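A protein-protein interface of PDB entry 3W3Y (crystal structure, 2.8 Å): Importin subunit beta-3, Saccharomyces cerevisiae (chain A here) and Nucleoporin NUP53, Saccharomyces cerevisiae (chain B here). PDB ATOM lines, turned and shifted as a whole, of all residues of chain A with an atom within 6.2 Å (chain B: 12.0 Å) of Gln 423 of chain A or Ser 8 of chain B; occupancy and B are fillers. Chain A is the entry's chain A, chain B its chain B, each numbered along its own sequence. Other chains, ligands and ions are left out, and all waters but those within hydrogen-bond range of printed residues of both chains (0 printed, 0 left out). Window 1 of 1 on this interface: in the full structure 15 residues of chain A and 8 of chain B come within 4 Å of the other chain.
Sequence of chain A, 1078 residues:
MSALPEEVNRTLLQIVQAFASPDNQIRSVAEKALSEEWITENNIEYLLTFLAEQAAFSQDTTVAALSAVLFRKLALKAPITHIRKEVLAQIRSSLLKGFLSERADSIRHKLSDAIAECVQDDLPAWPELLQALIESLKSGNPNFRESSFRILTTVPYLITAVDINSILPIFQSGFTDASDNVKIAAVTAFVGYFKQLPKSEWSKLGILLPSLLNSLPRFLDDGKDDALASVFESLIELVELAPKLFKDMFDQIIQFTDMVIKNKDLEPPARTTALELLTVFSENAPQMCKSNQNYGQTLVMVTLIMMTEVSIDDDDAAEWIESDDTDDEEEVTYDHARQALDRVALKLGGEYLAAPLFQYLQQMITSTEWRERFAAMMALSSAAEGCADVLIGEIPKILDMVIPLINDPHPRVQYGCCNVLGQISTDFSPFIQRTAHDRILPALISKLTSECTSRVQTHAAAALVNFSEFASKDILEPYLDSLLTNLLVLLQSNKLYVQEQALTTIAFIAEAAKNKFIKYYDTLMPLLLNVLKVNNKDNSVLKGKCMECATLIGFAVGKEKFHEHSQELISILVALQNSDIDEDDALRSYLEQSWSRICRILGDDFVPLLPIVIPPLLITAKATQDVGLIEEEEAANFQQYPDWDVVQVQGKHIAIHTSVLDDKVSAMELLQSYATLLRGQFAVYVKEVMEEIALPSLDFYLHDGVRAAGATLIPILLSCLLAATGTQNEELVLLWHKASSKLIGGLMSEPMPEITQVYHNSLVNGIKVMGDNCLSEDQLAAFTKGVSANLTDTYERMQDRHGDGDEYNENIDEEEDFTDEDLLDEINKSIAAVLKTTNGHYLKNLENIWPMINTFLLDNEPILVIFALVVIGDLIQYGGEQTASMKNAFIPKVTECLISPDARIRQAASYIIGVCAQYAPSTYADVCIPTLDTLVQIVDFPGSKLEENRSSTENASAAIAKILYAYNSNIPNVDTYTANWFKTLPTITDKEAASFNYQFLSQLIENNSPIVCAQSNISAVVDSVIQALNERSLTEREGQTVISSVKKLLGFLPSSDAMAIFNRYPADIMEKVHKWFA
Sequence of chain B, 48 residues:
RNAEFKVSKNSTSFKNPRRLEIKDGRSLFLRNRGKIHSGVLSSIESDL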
ATOM      1  N   ARG A 338     -27.292   6.254   6.403  1.00  0.00           N
ATOM      2  CA  ARG A 338     -27.233   7.582   5.832  1.00  0.00           C
ATOM      3  C   ARG A 338     -27.342   8.585   6.979  1.00  0.00           C
ATOM      4  O   ARG A 338     -26.471   9.391   7.166  1.00  0.00           O
ATOM      5  CB  ARG A 338     -28.349   7.788   4.836  1.00  0.00           C
ATOM      6  CG  ARG A 338     -28.599   6.579   3.952  1.00  0.00           C
ATOM      7  CD  ARG A 338     -29.383   6.964   2.706  1.00  0.00           C
ATOM      8  NE  ARG A 338     -28.875   8.234   2.220  1.00  0.00           N
ATOM      9  CZ  ARG A 338     -29.468   8.995   1.321  1.00  0.00           C
ATOM     10  NH1 ARG A 338     -30.630   8.644   0.800  1.00  0.00           N
ATOM     11  NH2 ARG A 338     -28.908  10.153   0.998  1.00  0.00           N
ATOM     12  N   LEU A 380     -21.874  10.318   0.063  1.00  0.00           N
ATOM     13  CA  LEU A 380     -21.416  11.668  -0.223  1.00  0.00           C
ATOM     14  C   LEU A 380     -22.581  12.610   0.014  1.00  0.00           C
ATOM     15  O   LEU A 380     -22.433  13.680   0.579  1.00  0.00           O
ATOM     16  CB  LEU A 380     -20.965  11.711  -1.688  1.00  0.00           C
ATOM     17  CG  LEU A 380     -20.384  12.989  -2.269  1.00  0.00           C
ATOM     18  CD1 LEU A 380     -19.590  13.757  -1.221  1.00  0.00           C
ATOM     19  CD2 LEU A 380     -19.510  12.619  -3.450  1.00  0.00           C
ATOM     20  N   SER A 381     -23.745  12.174  -0.442  1.00  0.00           N
ATOM     21  CA  SER A 381     -24.971  12.872  -0.287  1.00  0.00           C
ATOM     22  C   SER A 381     -25.236  13.131   1.181  1.00  0.00           C
ATOM     23  O   SER A 381     -25.638  14.252   1.535  1.00  0.00           O
ATOM     24  CB  SER A 381     -26.082  12.045  -0.877  1.00  0.00           C
ATOM     25  OG  SER A 381     -26.007  12.114  -2.292  1.00  0.00           O
ATOM     26  N   SER A 382     -24.993  12.137   2.043  1.00  0.00           N
ATOM     27  CA  SER A 382     -25.209  12.299   3.489  1.00  0.00           C
ATOM     28  C   SER A 382     -24.227  13.255   4.162  1.00  0.00           C
ATOM     29  O   SER A 382     -24.599  14.030   5.045  1.00  0.00           O
ATOM     30  CB  SER A 382     -25.123  10.959   4.184  1.00  0.00           C
ATOM     31  OG  SER A 382     -26.108  10.095   3.622  1.00  0.00           O
ATOM     32  N   ALA A 384     -22.262  15.578   2.664  1.00  0.00           N
ATOM     33  CA  ALA A 384     -21.843  16.771   1.963  1.00  0.00           C
ATOM     34  C   ALA A 384     -22.043  18.017   2.792  1.00  0.00           C
ATOM     35  O   ALA A 384     -21.177  18.877   2.832  1.00  0.00           O
ATOM     36  CB  ALA A 384     -22.557  16.887   0.617  1.00  0.00           C
ATOM     37  N   GLU A 385     -23.191  18.138   3.438  1.00  0.00           N
ATOM     38  CA  GLU A 385     -23.451  19.353   4.212  1.00  0.00           C
ATOM     39  C   GLU A 385     -22.478  19.497   5.372  1.00  0.00           C
ATOM     40  O   GLU A 385     -21.886  20.561   5.556  1.00  0.00           O
ATOM     41  CB  GLU A 385     -24.868  19.357   4.749  1.00  0.00           C
ATOM     42  CG  GLU A 385     -25.207  20.477   5.703  1.00  0.00           C
ATOM     43  CD  GLU A 385     -26.633  20.403   6.201  1.00  0.00           C
ATOM     44  OE1 GLU A 385     -27.380  19.440   5.928  1.00  0.00           O
ATOM     45  OE2 GLU A 385     -27.034  21.350   6.878  1.00  0.00           O
ATOM     46  N   CYS A 418     -27.811  11.141  -9.589  1.00  0.00           N
ATOM     47  CA  CYS A 418     -28.794  12.196  -9.616  1.00  0.00           C
ATOM     48  C   CYS A 418     -28.893  12.791  -8.207  1.00  0.00           C
ATOM     49  O   CYS A 418     -28.841  13.998  -8.015  1.00  0.00           O
ATOM     50  CB  CYS A 418     -30.126  11.625 -10.128  1.00  0.00           C
ATOM     51  SG  CYS A 418     -30.108  11.472 -11.942  1.00  0.00           S
ATOM     52  N   ASN A 419     -28.973  11.893  -7.237  1.00  0.00           N
ATOM     53  CA  ASN A 419     -29.122  12.243  -5.859  1.00  0.00           C
ATOM     54  C   ASN A 419     -27.991  13.141  -5.396  1.00  0.00           C
ATOM     55  O   ASN A 419     -28.250  14.158  -4.782  1.00  0.00           O
ATOM     56  CB  ASN A 419     -29.215  10.972  -5.011  1.00  0.00           C
ATOM     57  CG  ASN A 419     -29.743  11.230  -3.623  1.00  0.00           C
ATOM     58  OD1 ASN A 419     -30.956  11.174  -3.372  1.00  0.00           O
ATOM     59  ND2 ASN A 419     -28.840  11.565  -2.726  1.00  0.00           N
ATOM     60  N   VAL A 420     -26.753  12.815  -5.727  1.00  0.00           N
ATOM     61  CA  VAL A 420     -25.640  13.647  -5.284  1.00  0.00           C
ATOM     62  C   VAL A 420     -25.673  15.001  -5.903  1.00  0.00           C
ATOM     63  O   VAL A 420     -25.395  15.974  -5.247  1.00  0.00           O
ATOM     64  CB  VAL A 420     -24.285  13.085  -5.660  1.00  0.00           C
ATOM     65  CG1 VAL A 420     -23.264  13.523  -4.657  1.00  0.00           C
ATOM     66  CG2 VAL A 420     -24.338  11.589  -5.643  1.00  0.00           C
ATOM     67  N   LEU A 421     -25.982  15.067  -7.183  1.00  0.00           N
ATOM     68  CA  LEU A 421     -25.941  16.346  -7.862  1.00  0.00           C
ATOM     69  C   LEU A 421     -27.030  17.264  -7.311  1.00  0.00           C
ATOM     70  O   LEU A 421     -26.830  18.464  -7.136  1.00  0.00           O
ATOM     71  CB  LEU A 421     -26.030  16.133  -9.378  1.00  0.00           C
ATOM     72  CG  LEU A 421     -24.940  15.265 -10.005  1.00  0.00           C
ATOM     73  CD1 LEU A 421     -25.250  15.101 -11.483  1.00  0.00           C
ATOM     74  CD2 LEU A 421     -23.548  15.837  -9.795  1.00  0.00           C
ATOM     75  N   GLY A 422     -28.165  16.658  -6.992  1.00  0.00           N
ATOM     76  CA  GLY A 422     -29.222  17.305  -6.221  1.00  0.00           C
ATOM     77  C   GLY A 422     -28.749  17.753  -4.842  1.00  0.00           C
ATOM     78  O   GLY A 422     -28.896  18.928  -4.472  1.00  0.00           O
ATOM     79  N   GLN A 423     -28.172  16.842  -4.070  1.00  0.00           N
ATOM     80  CA  GLN A 423     -27.861  17.187  -2.696  1.00  0.00           C
ATOM     81  C   GLN A 423     -26.830  18.322  -2.603  1.00  0.00           C
ATOM     82  O   GLN A 423     -26.932  19.237  -1.762  1.00  0.00           O
ATOM     83  CB  GLN A 423     -27.447  15.955  -1.885  1.00  0.00           C
ATOM     84  CG  GLN A 423     -27.452  16.143  -0.373  1.00  0.00           C
ATOM     85  CD  GLN A 423     -28.794  16.627   0.167  1.00  0.00           C
ATOM     86  OE1 GLN A 423     -29.803  15.931   0.014  1.00  0.00           O
ATOM     87  NE2 GLN A 423     -28.818  17.826   0.789  1.00  0.00           N
ATOM     88  N   ILE A 424     -25.854  18.282  -3.484  1.00  0.00           N
ATOM     89  CA  ILE A 424     -24.832  19.261  -3.407  1.00  0.00           C
ATOM     90  C   ILE A 424     -25.280  20.572  -4.015  1.00  0.00           C
ATOM     91  O   ILE A 424     -24.766  21.621  -3.608  1.00  0.00           O
ATOM     92  CB  ILE A 424     -23.512  18.786  -3.997  1.00  0.00           C
ATOM     93  CG1 ILE A 424     -23.573  18.668  -5.520  1.00  0.00           C
ATOM     94  CG2 ILE A 424     -23.070  17.480  -3.347  1.00  0.00           C
ATOM     95  CD1 ILE A 424     -22.266  18.158  -6.120  1.00  0.00           C
ATOM     96  N   SER A 425     -26.239  20.559  -4.946  1.00  0.00           N
ATOM     97  CA  SER A 425     -26.775  21.832  -5.400  1.00  0.00           C
ATOM     98  C   SER A 425     -27.373  22.607  -4.227  1.00  0.00           C
ATOM     99  O   SER A 425     -27.353  23.851  -4.212  1.00  0.00           O
ATOM    100  CB  SER A 425     -27.796  21.660  -6.502  1.00  0.00           C
ATOM    101  OG  SER A 425     -27.131  21.056  -7.578  1.00  0.00           O
ATOM    102  N   THR A 426     -27.860  21.878  -3.226  1.00  0.00           N
ATOM    103  CA  THR A 426     -28.373  22.521  -2.037  1.00  0.00           C
ATOM    104  C   THR A 426     -27.239  22.910  -1.114  1.00  0.00           C
ATOM    105  O   THR A 426     -27.147  24.053  -0.676  1.00  0.00           O
ATOM    106  CB  THR A 426     -29.305  21.598  -1.261  1.00  0.00           C
ATOM    107  OG1 THR A 426     -30.429  21.268  -2.077  1.00  0.00           O
ATOM    108  CG2 THR A 426     -29.799  22.300  -0.024  1.00  0.00           C
ATOM    109  N   ASP A 427     -26.388  21.935  -0.823  1.00  0.00           N
ATOM    110  CA  ASP A 427     -25.451  22.070   0.260  1.00  0.00           C
ATOM    111  C   ASP A 427     -24.284  22.978  -0.052  1.00  0.00           C
ATOM    112  O   ASP A 427     -23.674  23.499   0.864  1.00  0.00           O
ATOM    113  CB  ASP A 427     -25.019  20.697   0.757  1.00  0.00           C
ATOM    114  CG  ASP A 427     -26.176  19.926   1.398  1.00  0.00           C
ATOM    115  OD1 ASP A 427     -27.005  20.562   2.103  1.00  0.00           O
ATOM    116  OD2 ASP A 427     -26.290  18.694   1.224  1.00  0.00           O
ATOM    117  N   PHE A 428     -23.974  23.189  -1.330  1.00  0.00           N
ATOM    118  CA  PHE A 428     -22.869  24.101  -1.690  1.00  0.00           C
ATOM    119  C   PHE A 428     -23.397  25.407  -2.330  1.00  0.00           C
ATOM    120  O   PHE A 428     -22.654  26.137  -2.984  1.00  0.00           O
ATOM    121  CB  PHE A 428     -21.796  23.409  -2.590  1.00  0.00           C
ATOM    122  CG  PHE A 428     -21.288  22.071  -2.064  1.00  0.00           C
ATOM    123  CD1 PHE A 428     -21.220  21.815  -0.698  1.00  0.00           C
ATOM    124  CD2 PHE A 428     -20.824  21.073  -2.940  1.00  0.00           C
ATOM    125  CE1 PHE A 428     -20.749  20.581  -0.237  1.00  0.00           C
ATOM    126  CE2 PHE A 428     -20.333  19.855  -2.471  1.00  0.00           C
ATOM    127  CZ  PHE A 428     -20.302  19.609  -1.122  1.00  0.00           C
ATOM    128  N   ALA A 463     -33.697  16.601  -8.803  1.00  0.00           N
ATOM    129  CA  ALA A 463     -32.439  17.282  -8.523  1.00  0.00           C
ATOM    130  C   ALA A 463     -32.417  18.665  -9.185  1.00  0.00           C
ATOM    131  O   ALA A 463     -31.642  19.556  -8.804  1.00  0.00           O
ATOM    132  CB  ALA A 463     -31.231  16.449  -8.947  1.00  0.00           C
ATOM    133  N   ASN A 466     -33.488  21.206  -6.595  1.00  0.00           N
ATOM    134  CA  ASN A 466     -32.412  21.680  -5.760  1.00  0.00           C
ATOM    135  C   ASN A 466     -31.615  22.734  -6.497  1.00  0.00           C
ATOM    136  O   ASN A 466     -31.356  23.780  -5.977  1.00  0.00           O
ATOM    137  CB  ASN A 466     -31.501  20.521  -5.329  1.00  0.00           C
ATOM    138  CG  ASN A 466     -32.239  19.447  -4.523  1.00  0.00           C
ATOM    139  OD1 ASN A 466     -33.022  18.650  -5.051  1.00  0.00           O
ATOM    140  ND2 ASN A 466     -31.980  19.422  -3.227  1.00  0.00           N
ATOM    141  N   PHE B   5     -41.316  15.877  -5.243  1.00  0.00           N
ATOM    142  CA  PHE B   5     -40.545  17.079  -4.854  1.00  0.00           C
ATOM    143  C   PHE B   5     -39.039  17.025  -5.137  1.00  0.00           C
ATOM    144  O   PHE B   5     -38.579  16.847  -6.252  1.00  0.00           O
ATOM    145  CB  PHE B   5     -40.735  17.379  -3.373  1.00  0.00           C
ATOM    146  CG  PHE B   5     -40.643  18.853  -3.055  1.00  0.00           C
ATOM    147  CD1 PHE B   5     -39.428  19.458  -2.699  1.00  0.00           C
ATOM    148  CD2 PHE B   5     -41.780  19.657  -3.141  1.00  0.00           C
ATOM    149  CE1 PHE B   5     -39.350  20.813  -2.442  1.00  0.00           C
ATOM    150  CE2 PHE B   5     -41.714  21.018  -2.873  1.00  0.00           C
ATOM    151  CZ  PHE B   5     -40.499  21.595  -2.523  1.00  0.00           C
ATOM    152  N   LYS B   6     -38.294  17.213  -4.069  1.00  0.00           N
ATOM    153  CA  LYS B   6     -36.871  17.549  -4.066  1.00  0.00           C
ATOM    154  C   LYS B   6     -35.931  16.327  -3.837  1.00  0.00           C
ATOM    155  O   LYS B   6     -36.395  15.183  -3.685  1.00  0.00           O
ATOM    156  CB  LYS B   6     -36.721  18.420  -2.844  1.00  0.00           C
ATOM    157  CG  LYS B   6     -35.960  19.702  -2.898  1.00  0.00           C
ATOM    158  CD  LYS B   6     -36.029  20.186  -1.442  1.00  0.00           C
ATOM    159  CE  LYS B   6     -36.454  21.628  -1.268  1.00  0.00           C
ATOM    160  NZ  LYS B   6     -35.243  22.436  -1.502  1.00  0.00           N
ATOM    161  N   VAL B   7     -34.617  16.591  -3.763  1.00  0.00           N
ATOM    162  CA  VAL B   7     -33.641  15.647  -3.198  1.00  0.00           C
ATOM    163  C   VAL B   7     -33.247  16.207  -1.853  1.00  0.00           C
ATOM    164  O   VAL B   7     -32.836  17.352  -1.772  1.00  0.00           O
ATOM    165  CB  VAL B   7     -32.424  15.414  -4.147  1.00  0.00           C
ATOM    166  CG1 VAL B   7     -31.129  14.937  -3.453  1.00  0.00           C
ATOM    167  CG2 VAL B   7     -32.853  14.416  -5.219  1.00  0.00           C
ATOM    168  N   SER B   8     -33.466  15.426  -0.796  1.00  0.00           N
ATOM    169  CA  SER B   8     -33.095  15.809   0.539  1.00  0.00           C
ATOM    170  C   SER B   8     -32.769  14.572   1.334  1.00  0.00           C
ATOM    171  O   SER B   8     -32.846  13.451   0.830  1.00  0.00           O
ATOM    172  CB  SER B   8     -34.225  16.580   1.254  1.00  0.00           C
ATOM    173  OG  SER B   8     -35.358  15.751   1.462  1.00  0.00           O
ATOM    174  N   LYS B   9     -32.426  14.794   2.604  1.00  0.00           N
ATOM    175  CA  LYS B   9     -32.112  13.727   3.522  1.00  0.00           C
ATOM    176  C   LYS B   9     -33.051  13.744   4.691  1.00  0.00           C
ATOM    177  O   LYS B   9     -33.134  14.754   5.369  1.00  0.00           O
ATOM    178  CB  LYS B   9     -30.694  13.865   4.039  1.00  0.00           C
ATOM    179  CG  LYS B   9     -30.039  15.230   3.934  1.00  0.00           C
ATOM    180  CD  LYS B   9     -28.583  15.117   4.384  1.00  0.00           C
ATOM    181  CE  LYS B   9     -28.037  16.475   4.861  1.00  0.00           C
ATOM    182  NZ  LYS B   9     -26.610  16.793   4.515  1.00  0.00           N
ATOM    183  N   ASN B  10     -33.769  12.647   4.935  1.00  0.00           N
ATOM    184  CA  ASN B  10     -34.655  12.606   6.100  1.00  0.00           C
ATOM    185  C   ASN B  10     -33.889  12.474   7.435  1.00  0.00           C
ATOM    186  O   ASN B  10     -32.650  12.418   7.478  1.00  0.00           O
ATOM    187  CB  ASN B  10     -35.770  11.550   5.959  1.00  0.00           C
ATOM    188  CG  ASN B  10     -35.235  10.180   5.613  1.00  0.00           C
ATOM    189  OD1 ASN B  10     -34.030   9.996   5.407  1.00  0.00           O
ATOM    190  ND2 ASN B  10     -36.131   9.205   5.549  1.00  0.00           N
ATOM    191  N   SER B  11     -34.658  12.481   8.521  1.00  0.00           N
ATOM    192  CA  SER B  11     -34.150  12.327   9.881  1.00  0.00           C
ATOM    193  C   SER B  11     -35.349  12.026  10.759  1.00  0.00           C
ATOM    194  O   SER B  11     -36.242  12.859  10.921  1.00  0.00           O
ATOM    195  CB  SER B  11     -33.408  13.576  10.350  1.00  0.00           C
ATOM    196  OG  SER B  11     -34.277  14.684  10.367  1.00  0.00           O
ATOM    197  N   THR B  12     -35.367  10.810  11.304  1.00  0.00           N
ATOM    198  CA  THR B  12     -36.575  10.257  11.904  1.00  0.00           C
ATOM    199  C   THR B  12     -36.334   9.791  13.349  1.00  0.00           C
ATOM    200  O   THR B  12     -35.238   9.358  13.707  1.00  0.00           O
ATOM    201  CB  THR B  12     -37.203   9.126  11.021  1.00  0.00           C
ATOM    202  OG1 THR B  12     -36.412   7.940  11.094  1.00  0.00           O
ATOM    203  CG2 THR B  12     -37.327   9.535   9.539  1.00  0.00           C
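The backbone carbonyl oxygen (O) of Ser 382 of chain A lies within hydrogen-bond range of the side-chain amino group (NZ) of Lys 9 of chain B (3.5 Å). NZ of Lys 9 of chain B is in salt-bridge range of OE1 of Glu 385 of chain A (3.1 Å). The side-chain carboxylate (OD2) of Asp 427 of chain A is in salt-bridge range of the side-chain amino group (NZ) of Lys 9 of chain B, at 3.8 Å. ND2 of Asn 466 of chain A sits at hydrogen-bond distance from O of Val 7 of chain B.
The side-chain hydroxyl (OG) of Ser 381 of chain A lies within hydrogen-bond range of the side-chain amide nitrogen (ND2) of Asn 419 of chain A. O of Gly 422 of chain A lies close to ND2 of Asn 466 of chain A, 3.4 Å away. The side-chain amide nitrogen (NE2) of Gln 423 of chain A sits at hydrogen-bond distance from the side-chain carboxylate (OD2) of Asp 427 of chain A (2.7 Å). The side-chain hydroxyl (OG1) of Thr 426 of chain A is in hydrogen-bond range of the side-chain amide nitrogen (ND2) of Asn 466 of chain A, at 2.7 Å.
Val 7 of chain B touches Asn 419 of chain A (CG1 to O, 3.3 Å). Gly 422 of chain A touches Val 7 of chain B. CG1 of Val 7 of chain B touches N of Gln 423 of chain A, at 3.6 Å. Gln 423 of chain A touches Ser 8 of chain B (OE1 to CA, 3.3 Å). N of Lys 9 of chain B touches OE1 of Gln 423 of chain A (3.9 Å). Asn 466 of chain A touches Lys 6 of chain B (OD1 to CG, 3.8 Å).
No residue of chain B comes within 4 Å of Ser 381 of chain A. Ser 382 of chain A touches just one residue of chain B: Lys 9. No residue of chain B comes within 4 Å of Ala 384 of chain A. Of the printed residues of chain B, Glu 385 of chain A touches Lys 9. Cys 418 of chain A touches none of the printed residues of chain B. Asn 419 of chain A touches just one residue of chain B: Val 7 (3.3 Å). No residue of chain B comes within 4 Å of Val 420 of chain A. Gly 422 of chain A touches one residue of chain B. Gln 423 of chain A touches three residues of chain B. Ile 424 of chain A touches none of the printed residues of chain B. No residue of chain B comes within 4 Å of Ser 425 of chain A. No residue of chain B comes within 4 Å of Thr 426 of chain A. Asp 427 of chain A touches just one residue of chain B: Lys 9 (3.8 Å). Asn 466 of chain A touches just these residues of chain B: Lys 6 and Val 7. Printed residues of chain A within 4 Å of Lys 6 of chain B: Asn 466 (3.8 Å). Of the printed residues of chain A, Lys 9 of chain B touches Ser 382 (3.5 Å), Glu 385 (3.1 Å), Gln 423 (3.9 Å) and Asp 427 (3.8 Å). Asn 10 of chain B touches none of the printed residues of chain A. The nearest residue of chain A that does not touch Ser 8 of chain B is Asn 466 of chain A (4.9 Å).
Hydrophobic or aromatic side chains of chain B within 4 Å of the printed part of chain A: Val 7. Of the 19 printed residues of chain A, 7 touch a printed residue of chain B. Printed residues of chain A that touch a printed residue of chain B: Ser 382, Glu 385, Asn 419, Gly 422, Gln 423, Asp 427 and Asn 466. Along chain A the printed residues that touch a printed residue of chain B span positions 382 to 466. Among the printed residues, Asp or Glu carboxylates within 4 Å of a Lys or Arg side-chain nitrogen of the other chain: Glu 385 of chain A with Lys 9 of chain B (3.1 Å) and Asp 427 of chain A with Lys 9 of chain B (3.8 Å).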
